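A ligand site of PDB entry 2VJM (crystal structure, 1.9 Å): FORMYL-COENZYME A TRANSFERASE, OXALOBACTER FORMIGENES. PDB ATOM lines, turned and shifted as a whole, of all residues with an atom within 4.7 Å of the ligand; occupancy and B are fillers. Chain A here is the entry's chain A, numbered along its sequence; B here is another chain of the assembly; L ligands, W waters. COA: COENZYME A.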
ATOM      1  N   HIS A  15     -14.277   8.192  -1.163  1.00  0.00           N
ATOM      2  CA  HIS A  15     -13.197   7.480  -0.482  1.00  0.00           C
ATOM      3  C   HIS A  15     -13.455   7.500   1.030  1.00  0.00           C
ATOM      4  O   HIS A  15     -14.365   8.172   1.514  1.00  0.00           O
ATOM      5  CB  HIS A  15     -11.840   8.116  -0.811  1.00  0.00           C
ATOM      6  CG  HIS A  15     -11.672   9.502  -0.276  1.00  0.00           C
ATOM      7  ND1 HIS A  15     -10.553   9.886   0.429  1.00  0.00           N
ATOM      8  CD2 HIS A  15     -12.480  10.587  -0.318  1.00  0.00           C
ATOM      9  CE1 HIS A  15     -10.667  11.149   0.794  1.00  0.00           C
ATOM     10  NE2 HIS A  15     -11.831  11.594   0.356  1.00  0.00           N
ATOM     11  N   VAL A  16     -12.630   6.752   1.762  1.00  0.00           N
ATOM     12  CA  VAL A  16     -12.766   6.590   3.226  1.00  0.00           C
ATOM     13  C   VAL A  16     -14.093   5.889   3.558  1.00  0.00           C
ATOM     14  O   VAL A  16     -14.337   4.791   3.056  1.00  0.00           O
ATOM     15  CB  VAL A  16     -12.534   7.937   3.984  1.00  0.00           C
ATOM     16  CG1 VAL A  16     -12.320   7.668   5.492  1.00  0.00           C
ATOM     17  CG2 VAL A  16     -11.349   8.680   3.391  1.00  0.00           C
ATOM     18  N   GLN A  17     -14.965   6.484   4.389  1.00  0.00           N
ATOM     19  CA  GLN A  17     -16.128   5.732   4.890  1.00  0.00           C
ATOM     20  C   GLN A  17     -17.496   6.270   4.481  1.00  0.00           C
ATOM     21  O   GLN A  17     -18.327   5.506   4.002  1.00  0.00           O
ATOM     22  CB  GLN A  17     -16.067   5.553   6.421  1.00  0.00           C
ATOM     23  CG  GLN A  17     -17.208   4.648   6.902  1.00  0.00           C
ATOM     24  CD  GLN A  17     -17.176   4.271   8.375  1.00  0.00           C
ATOM     25  OE1 GLN A  17     -18.214   3.951   8.951  1.00  0.00           O
ATOM     26  NE2 GLN A  17     -15.996   4.293   8.982  1.00  0.00           N
ATOM     27  N   ALA A  18     -17.736   7.570   4.687  1.00  0.00           N
ATOM     28  CA  ALA A  18     -19.069   8.147   4.506  1.00  0.00           C
ATOM     29  C   ALA A  18     -19.601   7.955   3.091  1.00  0.00           C
ATOM     30  O   ALA A  18     -20.681   7.381   2.873  1.00  0.00           O
ATOM     31  CB  ALA A  18     -19.071   9.622   4.865  1.00  0.00           C
ATOM     32  N   GLU A  37     -10.577   6.206  -8.622  1.00  0.00           N
ATOM     33  CA  GLU A  37      -9.540   6.171  -7.601  1.00  0.00           C
ATOM     34  C   GLU A  37      -8.230   6.800  -8.063  1.00  0.00           C
ATOM     35  O   GLU A  37      -7.924   6.814  -9.254  1.00  0.00           O
ATOM     36  CB  GLU A  37      -9.275   4.732  -7.164  1.00  0.00           C
ATOM     37  CG  GLU A  37     -10.517   4.029  -6.657  1.00  0.00           C
ATOM     38  CD  GLU A  37     -10.194   2.699  -6.026  1.00  0.00           C
ATOM     39  OE1 GLU A  37      -9.479   2.692  -4.998  1.00  0.00           O
ATOM     40  OE2 GLU A  37     -10.653   1.672  -6.566  1.00  0.00           O
ATOM     41  N   ARG A  38      -7.472   7.313  -7.101  1.00  0.00           N
ATOM     42  CA  ARG A  38      -6.173   7.906  -7.369  1.00  0.00           C
ATOM     43  C   ARG A  38      -5.238   6.829  -7.919  1.00  0.00           C
ATOM     44  O   ARG A  38      -5.275   5.676  -7.481  1.00  0.00           O
ATOM     45  CB  ARG A  38      -5.576   8.528  -6.105  1.00  0.00           C
ATOM     46  CG  ARG A  38      -5.007   9.926  -6.321  1.00  0.00           C
ATOM     47  CD  ARG A  38      -4.072  10.349  -5.196  1.00  0.00           C
ATOM     48  NE  ARG A  38      -4.354  11.710  -4.730  1.00  0.00           N
ATOM     49  CZ  ARG A  38      -5.259  12.019  -3.788  1.00  0.00           C
ATOM     50  NH1 ARG A  38      -5.422  13.281  -3.439  1.00  0.00           N
ATOM     51  NH2 ARG A  38      -5.997  11.074  -3.209  1.00  0.00           N
ATOM     52  N   MET A  44      -7.584   5.448   0.168  1.00  0.00           N
ATOM     53  CA  MET A  44      -6.677   5.254   1.309  1.00  0.00           C
ATOM     54  C   MET A  44      -7.024   4.079   2.243  1.00  0.00           C
ATOM     55  O   MET A  44      -6.141   3.547   2.911  1.00  0.00           O
ATOM     56  CB  MET A  44      -6.528   6.565   2.123  1.00  0.00           C
ATOM     57  CG  MET A  44      -7.806   7.087   2.783  1.00  0.00           C
ATOM     58  SD  MET A  44      -7.645   8.772   3.485  1.00  0.00           S
ATOM     59  CE  MET A  44      -7.550   9.808   2.020  1.00  0.00           C
ATOM     60  N   LEU A  72      -7.581   7.105 -12.201  1.00  0.00           N
ATOM     61  CA  LEU A  72      -7.702   8.327 -12.965  1.00  0.00           C
ATOM     62  C   LEU A  72      -6.993   9.490 -12.278  1.00  0.00           C
ATOM     63  O   LEU A  72      -7.281   9.792 -11.113  1.00  0.00           O
ATOM     64  CB  LEU A  72      -9.184   8.677 -13.190  1.00  0.00           C
ATOM     65  CG  LEU A  72      -9.513   9.813 -14.167  1.00  0.00           C
ATOM     66  CD1 LEU A  72      -8.958   9.532 -15.566  1.00  0.00           C
ATOM     67  CD2 LEU A  72     -11.007  10.030 -14.233  1.00  0.00           C
ATOM     68  N   ASP A  73      -6.065  10.118 -12.998  1.00  0.00           N
ATOM     69  CA  ASP A  73      -5.481  11.376 -12.567  1.00  0.00           C
ATOM     70  C   ASP A  73      -6.383  12.488 -13.098  1.00  0.00           C
ATOM     71  O   ASP A  73      -6.363  12.790 -14.305  1.00  0.00           O
ATOM     72  CB  ASP A  73      -4.050  11.536 -13.083  1.00  0.00           C
ATOM     73  CG  ASP A  73      -3.342  12.755 -12.503  1.00  0.00           C
ATOM     74  OD1 ASP A  73      -4.029  13.684 -11.996  1.00  0.00           O
ATOM     75  OD2 ASP A  73      -2.096  12.777 -12.542  1.00  0.00           O
ATOM     76  N   MET A  74      -7.183  13.083 -12.217  1.00  0.00           N
ATOM     77  CA  MET A  74      -8.184  14.074 -12.616  1.00  0.00           C
ATOM     78  C   MET A  74      -7.604  15.489 -12.796  1.00  0.00           C
ATOM     79  O   MET A  74      -8.308  16.388 -13.265  1.00  0.00           O
ATOM     80  CB  MET A  74      -9.340  14.093 -11.605  1.00  0.00           C
ATOM     81  CG  MET A  74     -10.115  12.770 -11.550  1.00  0.00           C
ATOM     82  SD  MET A  74     -11.484  12.746 -10.373  1.00  0.00           S
ATOM     83  CE  MET A  74     -10.615  12.709  -8.811  1.00  0.00           C
ATOM     84  N   LYS A  75      -6.338  15.687 -12.425  1.00  0.00           N
ATOM     85  CA  LYS A  75      -5.652  16.959 -12.655  1.00  0.00           C
ATOM     86  C   LYS A  75      -4.803  16.949 -13.950  1.00  0.00           C
ATOM     87  O   LYS A  75      -3.846  17.710 -14.072  1.00  0.00           O
ATOM     88  CB  LYS A  75      -4.805  17.330 -11.436  1.00  0.00           C
ATOM     89  CG  LYS A  75      -5.658  17.677 -10.218  1.00  0.00           C
ATOM     90  CD  LYS A  75      -4.837  18.123  -9.017  1.00  0.00           C
ATOM     91  CE  LYS A  75      -5.743  18.456  -7.832  1.00  0.00           C
ATOM     92  NZ  LYS A  75      -4.985  18.913  -6.622  1.00  0.00           N
ATOM     93  N   ASN A  96     -16.985  12.778  -1.611  1.00  0.00           N
ATOM     94  CA  ASN A  96     -16.692  13.258  -0.259  1.00  0.00           C
ATOM     95  C   ASN A  96     -15.234  13.688  -0.140  1.00  0.00           C
ATOM     96  O   ASN A  96     -14.506  13.275   0.761  1.00  0.00           O
ATOM     97  CB  ASN A  96     -17.116  12.247   0.839  1.00  0.00           C
ATOM     98  CG  ASN A  96     -16.307  10.969   0.823  1.00  0.00           C
ATOM     99  OD1 ASN A  96     -16.030  10.393  -0.229  1.00  0.00           O
ATOM    100  ND2 ASN A  96     -15.944  10.486   2.023  1.00  0.00           N
ATOM    101  N   PHE A  97     -14.844  14.540  -1.088  1.00  0.00           N
ATOM    102  CA  PHE A  97     -13.583  15.281  -0.997  1.00  0.00           C
ATOM    103  C   PHE A  97     -13.762  16.419   0.005  1.00  0.00           C
ATOM    104  O   PHE A  97     -14.858  16.653   0.511  1.00  0.00           O
ATOM    105  CB  PHE A  97     -13.209  15.896  -2.365  1.00  0.00           C
ATOM    106  CG  PHE A  97     -12.886  14.886  -3.432  1.00  0.00           C
ATOM    107  CD1 PHE A  97     -13.531  14.938  -4.664  1.00  0.00           C
ATOM    108  CD2 PHE A  97     -11.926  13.912  -3.227  1.00  0.00           C
ATOM    109  CE1 PHE A  97     -13.228  14.016  -5.666  1.00  0.00           C
ATOM    110  CE2 PHE A  97     -11.613  12.991  -4.232  1.00  0.00           C
ATOM    111  CZ  PHE A  97     -12.270  13.043  -5.439  1.00  0.00           C
ATOM    112  N   GLY A  98     -12.671  17.134   0.266  1.00  0.00           N
ATOM    113  CA  GLY A  98     -12.746  18.345   1.080  1.00  0.00           C
ATOM    114  C   GLY A  98     -13.565  19.420   0.409  1.00  0.00           C
ATOM    115  O   GLY A  98     -13.834  19.355  -0.798  1.00  0.00           O
ATOM    116  N   PRO A  99     -14.014  20.428   1.186  1.00  0.00           N
ATOM    117  CA  PRO A  99     -14.737  21.582   0.661  1.00  0.00           C
ATOM    118  C   PRO A  99     -14.079  22.226  -0.562  1.00  0.00           C
ATOM    119  O   PRO A  99     -12.882  22.538  -0.524  1.00  0.00           O
ATOM    120  CB  PRO A  99     -14.747  22.559   1.842  1.00  0.00           C
ATOM    121  CG  PRO A  99     -14.715  21.680   3.030  1.00  0.00           C
ATOM    122  CD  PRO A  99     -13.855  20.502   2.654  1.00  0.00           C
ATOM    123  N   ALA A 101     -13.136  21.015  -3.409  1.00  0.00           N
ATOM    124  CA  ALA A 101     -12.187  20.204  -4.190  1.00  0.00           C
ATOM    125  C   ALA A 101     -12.684  19.896  -5.604  1.00  0.00           C
ATOM    126  O   ALA A 101     -11.953  20.066  -6.573  1.00  0.00           O
ATOM    127  CB  ALA A 101     -11.860  18.901  -3.447  1.00  0.00           C
ATOM    128  N   ARG A 104     -12.675  23.080  -7.699  1.00  0.00           N
ATOM    129  CA  ARG A 104     -11.325  23.432  -8.140  1.00  0.00           C
ATOM    130  C   ARG A 104     -10.824  22.553  -9.293  1.00  0.00           C
ATOM    131  O   ARG A 104      -9.908  22.945 -10.003  1.00  0.00           O
ATOM    132  CB  ARG A 104     -10.348  23.378  -6.965  1.00  0.00           C
ATOM    133  CG  ARG A 104     -10.505  24.537  -5.985  1.00  0.00           C
ATOM    134  CD  ARG A 104      -9.388  24.557  -4.959  1.00  0.00           C
ATOM    135  NE  ARG A 104      -9.441  23.406  -4.065  1.00  0.00           N
ATOM    136  CZ  ARG A 104     -10.147  23.346  -2.933  1.00  0.00           C
ATOM    137  NH1 ARG A 104     -10.895  24.372  -2.532  1.00  0.00           N
ATOM    138  NH2 ARG A 104     -10.107  22.237  -2.208  1.00  0.00           N
ATOM    139  N   MET A 105     -11.432  21.379  -9.464  1.00  0.00           N
ATOM    140  CA  MET A 105     -11.169  20.538 -10.640  1.00  0.00           C
ATOM    141  C   MET A 105     -11.869  21.068 -11.897  1.00  0.00           C
ATOM    142  O   MET A 105     -11.581  20.611 -12.998  1.00  0.00           O
ATOM    143  CB  MET A 105     -11.613  19.084 -10.391  1.00  0.00           C
ATOM    144  CG  MET A 105     -10.614  18.259  -9.617  1.00  0.00           C
ATOM    145  SD  MET A 105     -11.245  16.611  -9.212  1.00  0.00           S
ATOM    146  CE  MET A 105      -9.802  15.896  -8.417  1.00  0.00           C
ATOM    147  N   VAL A 124     -20.991  14.620   0.640  1.00  0.00           N
ATOM    148  CA  VAL A 124     -20.847  14.586   2.091  1.00  0.00           C
ATOM    149  C   VAL A 124     -19.734  15.569   2.474  1.00  0.00           C
ATOM    150  O   VAL A 124     -18.633  15.514   1.920  1.00  0.00           O
ATOM    151  CB  VAL A 124     -20.460  13.206   2.647  1.00  0.00           C
ATOM    152  CG1 VAL A 124     -20.250  13.286   4.172  1.00  0.00           C
ATOM    153  CG2 VAL A 124     -21.520  12.177   2.309  1.00  0.00           C
ATOM    154  N   LYS A 125     -20.043  16.478   3.395  1.00  0.00           N
ATOM    155  CA  LYS A 125     -19.059  17.411   3.938  1.00  0.00           C
ATOM    156  C   LYS A 125     -19.155  17.389   5.469  1.00  0.00           C
ATOM    157  O   LYS A 125     -20.096  16.815   6.021  1.00  0.00           O
ATOM    158  CB  LYS A 125     -19.314  18.842   3.436  1.00  0.00           C
ATOM    159  CG  LYS A 125     -19.165  19.009   1.922  1.00  0.00           C
ATOM    160  CD  LYS A 125     -17.704  19.062   1.482  1.00  0.00           C
ATOM    161  CE  LYS A 125     -17.537  18.674   0.011  1.00  0.00           C
ATOM    162  NZ  LYS A 125     -17.494  17.194  -0.147  1.00  0.00           N
ATOM    163  N   GLY A 126     -18.171  17.980   6.135  1.00  0.00           N
ATOM    164  CA  GLY A 126     -18.167  18.057   7.590  1.00  0.00           C
ATOM    165  C   GLY A 126     -19.284  18.955   8.110  1.00  0.00           C
ATOM    166  O   GLY A 126     -20.059  18.551   9.001  1.00  0.00           O
ATOM    167  N   LYS A 137     -12.074  20.347   7.230  1.00  0.00           N
ATOM    168  CA  LYS A 137     -11.986  18.911   6.974  1.00  0.00           C
ATOM    169  C   LYS A 137     -12.282  18.166   8.277  1.00  0.00           C
ATOM    170  O   LYS A 137     -11.685  18.447   9.308  1.00  0.00           O
ATOM    171  CB  LYS A 137     -10.591  18.541   6.448  1.00  0.00           C
ATOM    172  CG  LYS A 137     -10.307  19.074   5.041  1.00  0.00           C
ATOM    173  CD  LYS A 137      -8.911  18.682   4.573  1.00  0.00           C
ATOM    174  CE  LYS A 137      -8.635  19.225   3.177  1.00  0.00           C
ATOM    175  NZ  LYS A 137      -7.294  18.796   2.660  1.00  0.00           N
ATOM    176  N   VAL A 138     -13.221  17.228   8.213  1.00  0.00           N
ATOM    177  CA  VAL A 138     -13.746  16.573   9.414  1.00  0.00           C
ATOM    178  C   VAL A 138     -13.616  15.064   9.309  1.00  0.00           C
ATOM    179  O   VAL A 138     -13.922  14.484   8.272  1.00  0.00           O
ATOM    180  CB  VAL A 138     -15.244  16.953   9.629  1.00  0.00           C
ATOM    181  CG1 VAL A 138     -15.848  16.164  10.776  1.00  0.00           C
ATOM    182  CG2 VAL A 138     -15.394  18.445   9.852  1.00  0.00           C
ATOM    183  N   TYR A 139     -13.156  14.428  10.399  1.00  0.00           N
ATOM    184  CA  TYR A 139     -13.116  12.975  10.506  1.00  0.00           C
ATOM    185  C   TYR A 139     -14.198  12.470  11.489  1.00  0.00           C
ATOM    186  O   TYR A 139     -14.803  13.270  12.210  1.00  0.00           O
ATOM    187  CB  TYR A 139     -11.721  12.509  10.956  1.00  0.00           C
ATOM    188  N   GLU A 140     -14.408  11.157  11.513  1.00  0.00           N
ATOM    189  CA  GLU A 140     -15.464  10.498  12.314  1.00  0.00           C
ATOM    190  C   GLU A 140     -15.714  11.124  13.691  1.00  0.00           C
ATOM    191  O   GLU A 140     -16.797  11.662  13.948  1.00  0.00           O
ATOM    192  CB  GLU A 140     -15.123   9.005  12.499  1.00  0.00           C
ATOM    193  CG  GLU A 140     -16.024   8.244  13.483  1.00  0.00           C
ATOM    194  CD  GLU A 140     -17.468   8.210  13.032  1.00  0.00           C
ATOM    195  OE1 GLU A 140     -18.360   8.503  13.855  1.00  0.00           O
ATOM    196  OE2 GLU A 140     -17.719   7.894  11.848  1.00  0.00           O
ATOM    197  N   ASP A 169     -19.549   8.990  10.022  1.00  0.00           N
ATOM    198  CA  ASP A 169     -19.274   8.581   8.636  1.00  0.00           C
ATOM    199  C   ASP A 169     -20.396   7.768   8.018  1.00  0.00           C
ATOM    200  O   ASP A 169     -21.123   8.282   7.182  1.00  0.00           O
ATOM    201  CB  ASP A 169     -17.951   7.816   8.579  1.00  0.00           C
ATOM    202  CG  ASP A 169     -16.828   8.819   8.524  1.00  0.00           C
ATOM    203  OD1 ASP A 169     -16.397   9.306   9.549  1.00  0.00           O
ATOM    204  N   MET A 200     -21.898  16.072   7.983  1.00  0.00           N
ATOM    205  CA  MET A 200     -21.682  15.106   9.061  1.00  0.00           C
ATOM    206  C   MET A 200     -22.244  15.612  10.395  1.00  0.00           C
ATOM    207  O   MET A 200     -22.853  14.848  11.152  1.00  0.00           O
ATOM    208  CB  MET A 200     -20.199  14.771   9.175  1.00  0.00           C
ATOM    209  CG  MET A 200     -19.632  14.055   7.935  1.00  0.00           C
ATOM    210  SD  MET A 200     -17.826  14.083   7.909  1.00  0.00           S
ATOM    211  CE  MET A 200     -17.492  12.720   9.006  1.00  0.00           C
ATOM    212  N   MET B 288      -0.588  14.175   8.320  1.00  0.00           N
ATOM    213  CA  MET B 288      -0.581  15.514   8.929  1.00  0.00           C
ATOM    214  C   MET B 288       0.486  15.698  10.014  1.00  0.00           C
ATOM    215  O   MET B 288       0.490  16.711  10.712  1.00  0.00           O
ATOM    216  CB  MET B 288      -1.968  15.833   9.516  1.00  0.00           C
ATOM    217  CG  MET B 288      -3.065  16.028   8.472  1.00  0.00           C
ATOM    218  SD  MET B 288      -3.055  17.677   7.739  1.00  0.00           S
ATOM    219  CE  MET B 288      -4.222  17.459   6.394  1.00  0.00           C
HETATM  220  N1A COA L   1      -6.759  12.750  -9.113  1.00  0.00           N
HETATM  221  C2A COA L   1      -6.341  14.009  -8.905  1.00  0.00           C
HETATM  222  N3A COA L   1      -6.610  14.651  -7.751  1.00  0.00           N
HETATM  223  C4A COA L   1      -7.315  14.037  -6.766  1.00  0.00           C
HETATM  224  C5A COA L   1      -7.754  12.736  -6.958  1.00  0.00           C
HETATM  225  C6A COA L   1      -7.470  12.090  -8.159  1.00  0.00           C
HETATM  226  N6A COA L   1      -7.877  10.839  -8.393  1.00  0.00           N
HETATM  227  N7A COA L   1      -8.419  12.384  -5.835  1.00  0.00           N
HETATM  228  C8A COA L   1      -8.385  13.434  -4.983  1.00  0.00           C
HETATM  229  N9A COA L   1      -7.706  14.442  -5.555  1.00  0.00           N
HETATM  230  C1B COA L   1      -7.420  15.782  -4.976  1.00  0.00           C
HETATM  231  C2B COA L   1      -8.666  16.518  -4.509  1.00  0.00           C
HETATM  232  O2B COA L   1      -9.404  17.097  -5.591  1.00  0.00           O
HETATM  233  C3B COA L   1      -8.069  17.551  -3.586  1.00  0.00           C
HETATM  234  O3B COA L   1      -7.692  18.683  -4.361  1.00  0.00           O
HETATM  235  P3B COA L   1      -7.357  20.138  -3.757  1.00  0.00           P
HETATM  236  O7A COA L   1      -7.909  20.154  -2.348  1.00  0.00           O
HETATM  237  O8A COA L   1      -5.865  20.327  -3.858  1.00  0.00           O
HETATM  238  O9A COA L   1      -7.968  21.101  -4.743  1.00  0.00           O
HETATM  239  C4B COA L   1      -6.826  16.884  -3.002  1.00  0.00           C
HETATM  240  O4B COA L   1      -6.596  15.721  -3.813  1.00  0.00           O
HETATM  241  C5B COA L   1      -6.968  16.529  -1.528  1.00  0.00           C
HETATM  242  O5B COA L   1      -8.055  15.605  -1.319  1.00  0.00           O
HETATM  243  P1A COA L   1      -9.118  15.840  -0.126  1.00  0.00           P
HETATM  244  O1A COA L   1      -9.935  14.586   0.102  1.00  0.00           O
HETATM  245  O2A COA L   1     -10.024  16.983  -0.512  1.00  0.00           O
HETATM  246  O3A COA L   1      -8.234  16.229   1.173  1.00  0.00           O
HETATM  247  P2A COA L   1      -7.637  15.198   2.275  1.00  0.00           P
HETATM  248  O4A COA L   1      -6.524  15.938   2.964  1.00  0.00           O
HETATM  249  O5A COA L   1      -7.359  13.856   1.656  1.00  0.00           O
HETATM  250  O6A COA L   1      -8.823  15.059   3.360  1.00  0.00           O
HETATM  251  CBP COA L   1     -10.923  14.152   4.177  1.00  0.00           C
HETATM  252  CCP COA L   1      -9.520  13.843   3.636  1.00  0.00           C
HETATM  253  CDP COA L   1     -11.675  12.846   4.393  1.00  0.00           C
HETATM  254  CEP COA L   1     -10.745  14.857   5.522  1.00  0.00           C
HETATM  255  CAP COA L   1     -11.652  15.051   3.168  1.00  0.00           C
HETATM  256  OAP COA L   1     -11.742  14.383   1.903  1.00  0.00           O
HETATM  257  C9P COA L   1     -13.035  15.436   3.643  1.00  0.00           C
HETATM  258  O9P COA L   1     -13.189  16.427   4.517  1.00  0.00           O
HETATM  259  N8P COA L   1     -14.075  14.751   3.176  1.00  0.00           N
HETATM  260  C7P COA L   1     -15.438  15.065   3.563  1.00  0.00           C
HETATM  261  C6P COA L   1     -15.806  14.535   4.944  1.00  0.00           C
HETATM  262  C5P COA L   1     -15.586  13.038   5.031  1.00  0.00           C
HETATM  263  O5P COA L   1     -16.004  12.284   4.131  1.00  0.00           O
HETATM  264  N4P COA L   1     -14.954  12.618   6.138  1.00  0.00           N
HETATM  265  C3P COA L   1     -14.286  11.325   6.258  1.00  0.00           C
HETATM  266  C2P COA L   1     -14.894  10.480   7.375  1.00  0.00           C
HETATM  267  S1P COA L   1     -16.075   9.328   6.749  1.00  0.00           S
HETATM  268  O   HOH W   1     -15.189  17.979   5.504  1.00  0.00           O
HETATM  269  O   HOH W   2      -9.254  19.654  -6.586  1.00  0.00           O
HETATM  270  O   HOH W   3      -9.473  19.525  -0.371  1.00  0.00           O
HETATM  271  O   HOH W   4      -9.602   9.970  -6.260  1.00  0.00           O
HETATM  272  O   HOH W   5      -3.723  15.692  -5.079  1.00  0.00           O
HETATM  273  O   HOH W   6      -2.933  14.556  -9.361  1.00  0.00           O
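NE of Arg 104 lies within salt-bridge range of O9A of the ligand, 2.8 Å away.
N1A of the ligand sits at hydrogen-bond distance from N of Met 74 (3.2 Å).
N8P of the ligand lies within hydrogen-bond range of O of Phe 97 (3.4 Å).
A sulfur (S1P) of the ligand lies close to the backbone NH (N) of Ala 18.
A ring nitrogen (NE2) of His 15 sits at hydrogen-bond distance from an oxygen (OAP) of the ligand (3.2 Å).
O2A of the ligand sits at hydrogen-bond distance from N of Gly 98 (2.8 Å).
NZ of Lys 75 is in salt-bridge range of O8A of the ligand (3.2 Å).
The backbone carbonyl oxygen of Asn 96 sits at hydrogen-bond distance from a nitrogen (N8P) of the ligand (2.9 Å).
An oxygen (O5P) of the ligand sits at hydrogen-bond distance from the side-chain amide nitrogen (ND2) of Asn 96 (2.8 Å).
CG of Asp 169 is bonded to S1P of the ligand, at 2.0 Å.
The backbone carbonyl oxygen of Leu 72 is in hydrogen-bond range of a nitrogen (N6A) of the ligand, 3.0 Å away.
A nitrogen (N4P) of the ligand sits close to the side-chain sulfur (SD) of Met 200, 3.7 Å away.
NH1 of Arg 38 is in hydrogen-bond range of O4B of the ligand, 2.7 Å away.
O of Val 138 sits at hydrogen-bond distance from N4P of the ligand, 3.0 Å away.
An oxygen (O4A) of the ligand is in salt-bridge range of the side-chain amino group (NZ) of Lys 137, at 3.0 Å.
The backbone NH (N) of Lys 75 sits at hydrogen-bond distance from the side-chain carboxylate (OD1) of Asp 73 (3.1 Å).
ND2 of Asn 96 lies within hydrogen-bond range of O of His 15 (2.8 Å).
O of Glu 37 lies within hydrogen-bond range of N of Leu 72, 3.0 Å away.
N of Met 200 sits at hydrogen-bond distance from O of Lys 125.
NZ of Lys 125 sits at hydrogen-bond distance from O of Phe 97 (2.8 Å).
OE2 of Glu 140 is in hydrogen-bond range of N of Asp 169 (2.8 Å).
NH2 of Arg 104 lies within hydrogen-bond range of O of Pro 99, at 3.3 Å.
The backbone carbonyl oxygen (O) of Gly 126 is in hydrogen-bond range of the backbone NH (N) of Met 200, 3.3 Å away.
Merely in contact with the ligand: Met 105, Val 124, Ala 101, Gln 17 and Asp 73.
Hydrophobic or aromatic side chains within 4 Å of the ligand: His 15, Ala 18, Met 74, Phe 97, Ala 101, Met 105 and Met 200.
The nearest printed residue that does not touch the ligand is Glu 37 (4.1 Å).
Water W3 lies within hydrogen-bond range of O7A of the ligand (2.6 Å) and NH2 of Arg 104 (3.3 Å).
Water W2 lies within hydrogen-bond range of an oxygen (O9A) of the ligand (2.7 Å) and the backbone carbonyl oxygen (O) of Ala 101 (2.7 Å).
Water W1 lies within hydrogen-bond range of an oxygen (O9P) of the ligand (2.7 Å), the backbone NH (N) of Gly 126 (3.0 Å) and the backbone NH (N) of Val 138 (3.4 Å).
Water W5 lies within hydrogen-bond range of O4B of the ligand and NH1 of Arg 38.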
